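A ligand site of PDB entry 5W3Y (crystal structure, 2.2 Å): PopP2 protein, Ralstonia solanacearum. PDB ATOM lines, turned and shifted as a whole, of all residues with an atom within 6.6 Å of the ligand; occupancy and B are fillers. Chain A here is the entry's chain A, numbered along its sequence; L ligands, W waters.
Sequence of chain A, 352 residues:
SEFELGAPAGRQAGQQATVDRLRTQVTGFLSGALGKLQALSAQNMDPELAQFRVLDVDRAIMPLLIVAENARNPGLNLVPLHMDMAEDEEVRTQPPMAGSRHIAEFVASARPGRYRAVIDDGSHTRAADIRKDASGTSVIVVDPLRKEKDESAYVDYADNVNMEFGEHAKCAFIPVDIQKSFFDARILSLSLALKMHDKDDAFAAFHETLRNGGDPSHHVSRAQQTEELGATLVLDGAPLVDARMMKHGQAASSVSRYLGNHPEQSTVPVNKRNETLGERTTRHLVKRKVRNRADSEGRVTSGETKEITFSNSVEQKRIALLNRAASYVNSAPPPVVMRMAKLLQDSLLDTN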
ATOM      1  N   ASP A  46      -7.243  13.272   6.090  1.00  0.00           N
ATOM      2  CA  ASP A  46      -7.351  14.693   5.823  1.00  0.00           C
ATOM      3  C   ASP A  46      -8.800  15.058   5.518  1.00  0.00           C
ATOM      4  O   ASP A  46      -9.457  14.407   4.705  1.00  0.00           O
ATOM      5  CB  ASP A  46      -6.455  15.107   4.661  1.00  0.00           C
ATOM      6  CG  ASP A  46      -6.687  16.536   4.241  1.00  0.00           C
ATOM      7  OD1 ASP A  46      -6.168  17.431   4.937  1.00  0.00           O
ATOM      8  OD2 ASP A  46      -7.379  16.761   3.221  1.00  0.00           O
ATOM      9  N   LYS A 180       0.211  25.542   8.299  1.00  0.00           N
ATOM     10  CA  LYS A 180       0.644  25.072   6.980  1.00  0.00           C
ATOM     11  C   LYS A 180      -0.592  24.699   6.141  1.00  0.00           C
ATOM     12  O   LYS A 180      -0.561  24.767   4.910  1.00  0.00           O
ATOM     13  CB  LYS A 180       1.584  23.875   7.085  1.00  0.00           C
ATOM     14  CG  LYS A 180       2.974  24.191   7.620  1.00  0.00           C
ATOM     15  CD  LYS A 180       3.678  25.301   6.843  1.00  0.00           C
ATOM     16  CE  LYS A 180       5.060  25.554   7.440  1.00  0.00           C
ATOM     17  NZ  LYS A 180       5.715  26.780   6.912  1.00  0.00           N
ATOM     18  N   SER A 181      -1.664  24.308   6.812  1.00  0.00           N
ATOM     19  CA  SER A 181      -2.875  23.909   6.095  1.00  0.00           C
ATOM     20  C   SER A 181      -3.670  25.130   5.677  1.00  0.00           C
ATOM     21  O   SER A 181      -3.409  26.241   6.121  1.00  0.00           O
ATOM     22  CB  SER A 181      -3.753  22.990   6.942  1.00  0.00           C
ATOM     23  OG  SER A 181      -4.722  23.728   7.659  1.00  0.00           O
ATOM     24  N   PHE A 182      -4.666  24.908   4.837  1.00  0.00           N
ATOM     25  CA  PHE A 182      -5.439  25.997   4.297  1.00  0.00           C
ATOM     26  C   PHE A 182      -6.548  26.430   5.250  1.00  0.00           C
ATOM     27  O   PHE A 182      -6.991  27.577   5.206  1.00  0.00           O
ATOM     28  CB  PHE A 182      -6.024  25.570   2.949  1.00  0.00           C
ATOM     29  CG  PHE A 182      -6.940  26.592   2.340  1.00  0.00           C
ATOM     30  CD1 PHE A 182      -6.424  27.682   1.661  1.00  0.00           C
ATOM     31  CD2 PHE A 182      -8.309  26.452   2.440  1.00  0.00           C
ATOM     32  CE1 PHE A 182      -7.260  28.630   1.100  1.00  0.00           C
ATOM     33  CE2 PHE A 182      -9.160  27.390   1.879  1.00  0.00           C
ATOM     34  CZ  PHE A 182      -8.639  28.472   1.210  1.00  0.00           C
ATOM     35  N   PHE A 183      -6.980  25.533   6.124  1.00  0.00           N
ATOM     36  CA  PHE A 183      -8.214  25.750   6.876  1.00  0.00           C
ATOM     37  C   PHE A 183      -8.079  25.947   8.403  1.00  0.00           C
ATOM     38  O   PHE A 183      -9.088  26.078   9.092  1.00  0.00           O
ATOM     39  CB  PHE A 183      -9.168  24.577   6.613  1.00  0.00           C
ATOM     40  CG  PHE A 183      -8.532  23.225   6.748  1.00  0.00           C
ATOM     41  CD1 PHE A 183      -8.422  22.612   7.996  1.00  0.00           C
ATOM     42  CD2 PHE A 183      -8.061  22.546   5.642  1.00  0.00           C
ATOM     43  CE1 PHE A 183      -7.839  21.347   8.130  1.00  0.00           C
ATOM     44  CE2 PHE A 183      -7.474  21.286   5.767  1.00  0.00           C
ATOM     45  CZ  PHE A 183      -7.365  20.697   7.015  1.00  0.00           C
ATOM     46  N   ASP A 184      -6.852  25.960   8.919  1.00  0.00           N
ATOM     47  CA  ASP A 184      -6.648  25.929  10.380  1.00  0.00           C
ATOM     48  C   ASP A 184      -6.451  27.303  11.059  1.00  0.00           C
ATOM     49  O   ASP A 184      -6.196  27.376  12.267  1.00  0.00           O
ATOM     50  CB  ASP A 184      -5.452  25.012  10.709  1.00  0.00           C
ATOM     51  CG  ASP A 184      -5.773  23.531  10.518  1.00  0.00           C
ATOM     52  OD1 ASP A 184      -6.907  23.113  10.862  1.00  0.00           O
ATOM     53  OD2 ASP A 184      -4.940  22.771   9.995  1.00  0.00           O
ATOM     54  N   GLN A 250       2.359  23.060  12.633  1.00  0.00           N
ATOM     55  CA  GLN A 250       1.934  21.935  11.808  1.00  0.00           C
ATOM     56  C   GLN A 250       3.123  21.240  11.169  1.00  0.00           C
ATOM     57  O   GLN A 250       3.195  20.001  11.172  1.00  0.00           O
ATOM     58  CB  GLN A 250       0.916  22.410  10.768  1.00  0.00           C
ATOM     59  CG  GLN A 250      -0.292  23.071  11.429  1.00  0.00           C
ATOM     60  CD  GLN A 250      -1.485  23.183  10.504  1.00  0.00           C
ATOM     61  OE1 GLN A 250      -1.506  24.001   9.581  1.00  0.00           O
ATOM     62  NE2 GLN A 250      -2.500  22.372  10.753  1.00  0.00           N
ATOM     63  N   ALA A 251       4.084  22.015  10.678  1.00  0.00           N
ATOM     64  CA  ALA A 251       5.283  21.406  10.091  1.00  0.00           C
ATOM     65  C   ALA A 251       6.337  21.153  11.169  1.00  0.00           C
ATOM     66  O   ALA A 251       6.707  22.064  11.913  1.00  0.00           O
ATOM     67  CB  ALA A 251       5.867  22.285   8.984  1.00  0.00           C
ATOM     68  N   ALA A 252       6.810  19.921  11.219  1.00  0.00           N
ATOM     69  CA  ALA A 252       7.886  19.533  12.123  1.00  0.00           C
ATOM     70  C   ALA A 252       9.085  20.458  11.986  1.00  0.00           C
ATOM     71  O   ALA A 252       9.750  20.801  12.969  1.00  0.00           O
ATOM     72  CB  ALA A 252       8.305  18.086  11.870  1.00  0.00           C
ATOM     73  N   SER A 253       9.364  20.863  10.748  1.00  0.00           N
ATOM     74  CA  SER A 253      10.497  21.745  10.495  1.00  0.00           C
ATOM     75  C   SER A 253      10.298  23.137  11.106  1.00  0.00           C
ATOM     76  O   SER A 253      11.264  23.789  11.488  1.00  0.00           O
ATOM     77  CB  SER A 253      10.760  21.830   8.989  1.00  0.00           C
ATOM     78  OG  SER A 253       9.630  22.294   8.285  1.00  0.00           O
ATOM     79  N   SER A 254       9.048  23.604  11.185  1.00  0.00           N
ATOM     80  CA  SER A 254       8.797  24.902  11.807  1.00  0.00           C
ATOM     81  C   SER A 254       9.155  24.862  13.299  1.00  0.00           C
ATOM     82  O   SER A 254       9.825  25.767  13.813  1.00  0.00           O
ATOM     83  CB  SER A 254       7.332  25.334  11.629  1.00  0.00           C
ATOM     84  OG  SER A 254       6.995  25.500  10.253  1.00  0.00           O
ATOM     85  N   ARG A 257      13.011  24.338  13.564  1.00  0.00           N
ATOM     86  CA  ARG A 257      13.722  25.556  13.195  1.00  0.00           C
ATOM     87  C   ARG A 257      13.641  26.607  14.281  1.00  0.00           C
ATOM     88  O   ARG A 257      14.626  27.303  14.572  1.00  0.00           O
ATOM     89  CB  ARG A 257      13.193  26.137  11.890  1.00  0.00           C
ATOM     90  CG  ARG A 257      13.919  27.371  11.400  1.00  0.00           C
ATOM     91  CD  ARG A 257      13.379  27.809  10.037  1.00  0.00           C
ATOM     92  NE  ARG A 257      13.477  26.745   9.039  1.00  0.00           N
ATOM     93  CZ  ARG A 257      12.431  26.128   8.503  1.00  0.00           C
ATOM     94  NH1 ARG A 257      12.617  25.169   7.590  1.00  0.00           N
ATOM     95  NH2 ARG A 257      11.202  26.461   8.852  1.00  0.00           N
ATOM     96  N   VAL A 290      -2.686  14.646   1.664  1.00  0.00           N
ATOM     97  CA  VAL A 290      -3.284  15.950   1.829  1.00  0.00           C
ATOM     98  C   VAL A 290      -3.465  16.494   0.398  1.00  0.00           C
ATOM     99  O   VAL A 290      -2.838  15.979  -0.533  1.00  0.00           O
ATOM    100  CB  VAL A 290      -2.378  16.841   2.742  1.00  0.00           C
ATOM    101  CG1 VAL A 290      -2.137  18.227   2.179  1.00  0.00           C
ATOM    102  CG2 VAL A 290      -2.950  16.898   4.166  1.00  0.00           C
ATOM    103  N   ARG A 291      -4.341  17.479   0.183  1.00  0.00           N
ATOM    104  CA  ARG A 291      -4.481  18.072  -1.152  1.00  0.00           C
ATOM    105  C   ARG A 291      -3.271  18.935  -1.477  1.00  0.00           C
ATOM    106  O   ARG A 291      -2.767  19.651  -0.615  1.00  0.00           O
ATOM    107  CB  ARG A 291      -5.769  18.907  -1.249  1.00  0.00           C
ATOM    108  N   ASN A 292      -2.796  18.891  -2.718  1.00  0.00           N
ATOM    109  CA  ASN A 292      -1.652  19.715  -3.108  1.00  0.00           C
ATOM    110  C   ASN A 292      -2.073  21.056  -3.715  1.00  0.00           C
ATOM    111  O   ASN A 292      -2.872  21.094  -4.653  1.00  0.00           O
ATOM    112  CB  ASN A 292      -0.771  18.965  -4.108  1.00  0.00           C
ATOM    113  CG  ASN A 292       0.653  19.508  -4.173  1.00  0.00           C
ATOM    114  OD1 ASN A 292       0.934  20.610  -3.688  1.00  0.00           O
ATOM    115  ND2 ASN A 292       1.548  18.753  -4.799  1.00  0.00           N
ATOM    116  N   ARG A 293      -1.539  22.154  -3.186  1.00  0.00           N
ATOM    117  CA  ARG A 293      -1.853  23.479  -3.714  1.00  0.00           C
ATOM    118  C   ARG A 293      -0.610  24.359  -3.706  1.00  0.00           C
ATOM    119  O   ARG A 293      -0.043  24.665  -4.750  1.00  0.00           O
ATOM    120  CB  ARG A 293      -2.990  24.162  -2.946  1.00  0.00           C
ATOM    121  CG  ARG A 293      -2.907  24.087  -1.431  1.00  0.00           C
ATOM    122  CD  ARG A 293      -3.957  25.001  -0.767  1.00  0.00           C
ATOM    123  NE  ARG A 293      -5.353  24.686  -1.059  1.00  0.00           N
ATOM    124  CZ  ARG A 293      -6.089  23.825  -0.372  1.00  0.00           C
ATOM    125  NH1 ARG A 293      -7.354  23.615  -0.704  1.00  0.00           N
ATOM    126  NH2 ARG A 293      -5.576  23.169   0.663  1.00  0.00           N
ATOM    127  N   LYS A 306      -0.725  14.797  -2.143  1.00  0.00           N
ATOM    128  CA  LYS A 306       0.672  14.633  -1.791  1.00  0.00           C
ATOM    129  C   LYS A 306       0.745  14.101  -0.356  1.00  0.00           C
ATOM    130  O   LYS A 306      -0.063  14.477   0.500  1.00  0.00           O
ATOM    131  CB  LYS A 306       1.441  15.958  -1.915  1.00  0.00           C
ATOM    132  CG  LYS A 306       0.984  17.045  -0.951  1.00  0.00           C
ATOM    133  CD  LYS A 306       2.028  18.150  -0.804  1.00  0.00           C
ATOM    134  CE  LYS A 306       1.415  19.390  -0.164  1.00  0.00           C
ATOM    135  NZ  LYS A 306       2.394  20.512  -0.039  1.00  0.00           N
ATOM    136  N   GLU A 307       1.681  13.196  -0.119  1.00  0.00           N
ATOM    137  CA  GLU A 307       1.815  12.579   1.200  1.00  0.00           C
ATOM    138  C   GLU A 307       2.880  13.291   2.031  1.00  0.00           C
ATOM    139  O   GLU A 307       4.017  13.486   1.580  1.00  0.00           O
ATOM    140  CB  GLU A 307       2.140  11.093   1.078  1.00  0.00           C
ATOM    141  CG  GLU A 307       1.806  10.322   2.338  1.00  0.00           C
ATOM    142  CD  GLU A 307       2.255   8.878   2.274  1.00  0.00           C
ATOM    143  OE1 GLU A 307       3.443   8.627   1.999  1.00  0.00           O
ATOM    144  OE2 GLU A 307       1.399   7.993   2.484  1.00  0.00           O
ATOM    145  N   ILE A 308       2.506  13.692   3.230  1.00  0.00           N
ATOM    146  CA  ILE A 308       3.400  14.444   4.099  1.00  0.00           C
ATOM    147  C   ILE A 308       3.366  13.943   5.525  1.00  0.00           C
ATOM    148  O   ILE A 308       2.426  13.264   5.955  1.00  0.00           O
ATOM    149  CB  ILE A 308       3.069  15.944   4.091  1.00  0.00           C
ATOM    150  CG1 ILE A 308       1.584  16.151   4.373  1.00  0.00           C
ATOM    151  CG2 ILE A 308       3.392  16.564   2.768  1.00  0.00           C
ATOM    152  CD1 ILE A 308       1.200  17.596   4.358  1.00  0.00           C
ATOM    153  N   THR A 309       4.416  14.284   6.258  1.00  0.00           N
ATOM    154  CA  THR A 309       4.497  14.006   7.675  1.00  0.00           C
ATOM    155  C   THR A 309       4.413  15.324   8.411  1.00  0.00           C
ATOM    156  O   THR A 309       5.201  16.230   8.156  1.00  0.00           O
ATOM    157  CB  THR A 309       5.815  13.303   8.042  1.00  0.00           C
ATOM    158  OG1 THR A 309       5.886  12.023   7.419  1.00  0.00           O
ATOM    159  CG2 THR A 309       5.918  13.139   9.555  1.00  0.00           C
ATOM    160  N   PHE A 310       3.427  15.437   9.287  1.00  0.00           N
ATOM    161  CA  PHE A 310       3.210  16.683   9.995  1.00  0.00           C
ATOM    162  C   PHE A 310       2.531  16.432  11.349  1.00  0.00           C
ATOM    163  O   PHE A 310       2.116  15.311  11.666  1.00  0.00           O
ATOM    164  CB  PHE A 310       2.351  17.632   9.178  1.00  0.00           C
ATOM    165  CG  PHE A 310       0.914  17.214   9.057  1.00  0.00           C
ATOM    166  CD1 PHE A 310       0.515  16.296   8.111  1.00  0.00           C
ATOM    167  CD2 PHE A 310      -0.038  17.750   9.907  1.00  0.00           C
ATOM    168  CE1 PHE A 310      -0.817  15.928   8.006  1.00  0.00           C
ATOM    169  CE2 PHE A 310      -1.372  17.386   9.816  1.00  0.00           C
ATOM    170  CZ  PHE A 310      -1.754  16.473   8.856  1.00  0.00           C
ATOM    171  N   SER A 311       2.407  17.494  12.138  1.00  0.00           N
ATOM    172  CA  SER A 311       1.783  17.406  13.446  1.00  0.00           C
ATOM    173  C   SER A 311       0.266  17.605  13.363  1.00  0.00           C
ATOM    174  O   SER A 311      -0.204  18.583  12.807  1.00  0.00           O
ATOM    175  CB  SER A 311       2.384  18.437  14.389  1.00  0.00           C
ATOM    176  OG  SER A 311       1.637  18.549  15.587  1.00  0.00           O
HETATM  177  N1  LIG L   1      -1.104  20.288   6.598  1.00  0.00           N
HETATM  178  C1  LIG L   1      -0.028  20.154   7.431  1.00  0.00           C
HETATM  179  N2  LIG L   1       1.286  20.301   7.211  1.00  0.00           N
HETATM  180  C2  LIG L   1       1.548  20.641   5.892  1.00  0.00           C
HETATM  181  C3  LIG L   1       0.539  20.812   4.902  1.00  0.00           C
HETATM  182  C4  LIG L   1      -0.792  20.625   5.302  1.00  0.00           C
HETATM  183  N3  LIG L   1      -1.806  20.775   4.384  1.00  0.00           N
HETATM  184  N4  LIG L   1       1.102  21.149   3.663  1.00  0.00           N
HETATM  185  C5  LIG L   1       2.413  21.179   3.920  1.00  0.00           C
HETATM  186  N5  LIG L   1       2.741  20.878   5.244  1.00  0.00           N
HETATM  187  C6  LIG L   1       4.083  20.839   5.835  1.00  0.00           C
HETATM  188  C7  LIG L   1       4.844  19.585   5.331  1.00  0.00           C
HETATM  189  O1  LIG L   1       4.695  18.530   6.192  1.00  0.00           O
HETATM  190  C8  LIG L   1       6.308  20.136   5.425  1.00  0.00           C
HETATM  191  O2  LIG L   1       6.781  19.982   6.676  1.00  0.00           O
HETATM  192  P1  LIG L   1       8.567  19.480   6.660  1.00  0.00           P
HETATM  193  O3  LIG L   1       8.388  18.299   5.737  1.00  0.00           O
HETATM  194  O4  LIG L   1       9.286  20.710   6.103  1.00  0.00           O
HETATM  195  O5  LIG L   1       8.733  19.140   8.120  1.00  0.00           O
HETATM  196  C9  LIG L   1       6.126  21.644   5.109  1.00  0.00           C
HETATM  197  O6  LIG L   1       4.745  22.000   5.349  1.00  0.00           O
HETATM  198  C10 LIG L   1       6.519  21.893   3.656  1.00  0.00           C
HETATM  199  O7  LIG L   1       5.391  21.746   2.843  1.00  0.00           O
HETATM  200  P2  LIG L   1       5.968  20.989   1.498  1.00  0.00           P
HETATM  201  O8  LIG L   1       5.164  19.762   1.301  1.00  0.00           O
HETATM  202  O9  LIG L   1       7.471  20.932   1.428  1.00  0.00           O
HETATM  203  O10 LIG L   1       5.484  21.839   0.139  1.00  0.00           O
HETATM  204  P3  LIG L   1       5.955  23.367   0.205  1.00  0.00           P
HETATM  205  O11 LIG L   1       5.502  24.183  -0.985  1.00  0.00           O
HETATM  206  O12 LIG L   1       7.328  23.465   0.763  1.00  0.00           O
HETATM  207  O13 LIG L   1       5.041  24.086   1.505  1.00  0.00           O
HETATM  208  O   HOH W   1      -3.542  19.244   7.759  1.00  0.00           O
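OG of Ser 253 lies within hydrogen-bond range of O4 of the ligand (2.7 Å).
N of Ser 253 sits at hydrogen-bond distance from O5 of the ligand, at 3.2 Å.
NZ of Lys 306 is in salt-bridge range of O8 of the ligand, at 3.2 Å.
O of Thr 309 lies within hydrogen-bond range of O1 of the ligand.
Merely in contact with the ligand: Ile 308 (3.3 Å), Val 290 (3.4 Å), Ala 251 (3.4 Å), Lys 180 (3.4 Å), Phe 310 (3.5 Å), Ser 181 (3.7 Å) and Ala 252 (3.7 Å).
Hydrophobic or aromatic side chains that line the ligand: Ala 251, Ala 252, Val 290, Ile 308 and Phe 310.
The nearest printed residue that does not touch the ligand is Gln 250 (4.1 Å).
The backbone NH of Phe 183 sits at hydrogen-bond distance from the side-chain hydroxyl of Ser 181, 3.3 Å away.
The backbone carbonyl oxygen (O) of Lys 306 is in hydrogen-bond range of the backbone NH (N) of Val 290 (2.9 Å).
OE1 of Gln 250 is in hydrogen-bond range of N of Ser 181 (2.8 Å).
N of Lys 180 lies within hydrogen-bond range of OE1 of Gln 250 (2.6 Å).
OG of Ser 181 sits at hydrogen-bond distance from OD2 of Asp 184 (2.5 Å).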
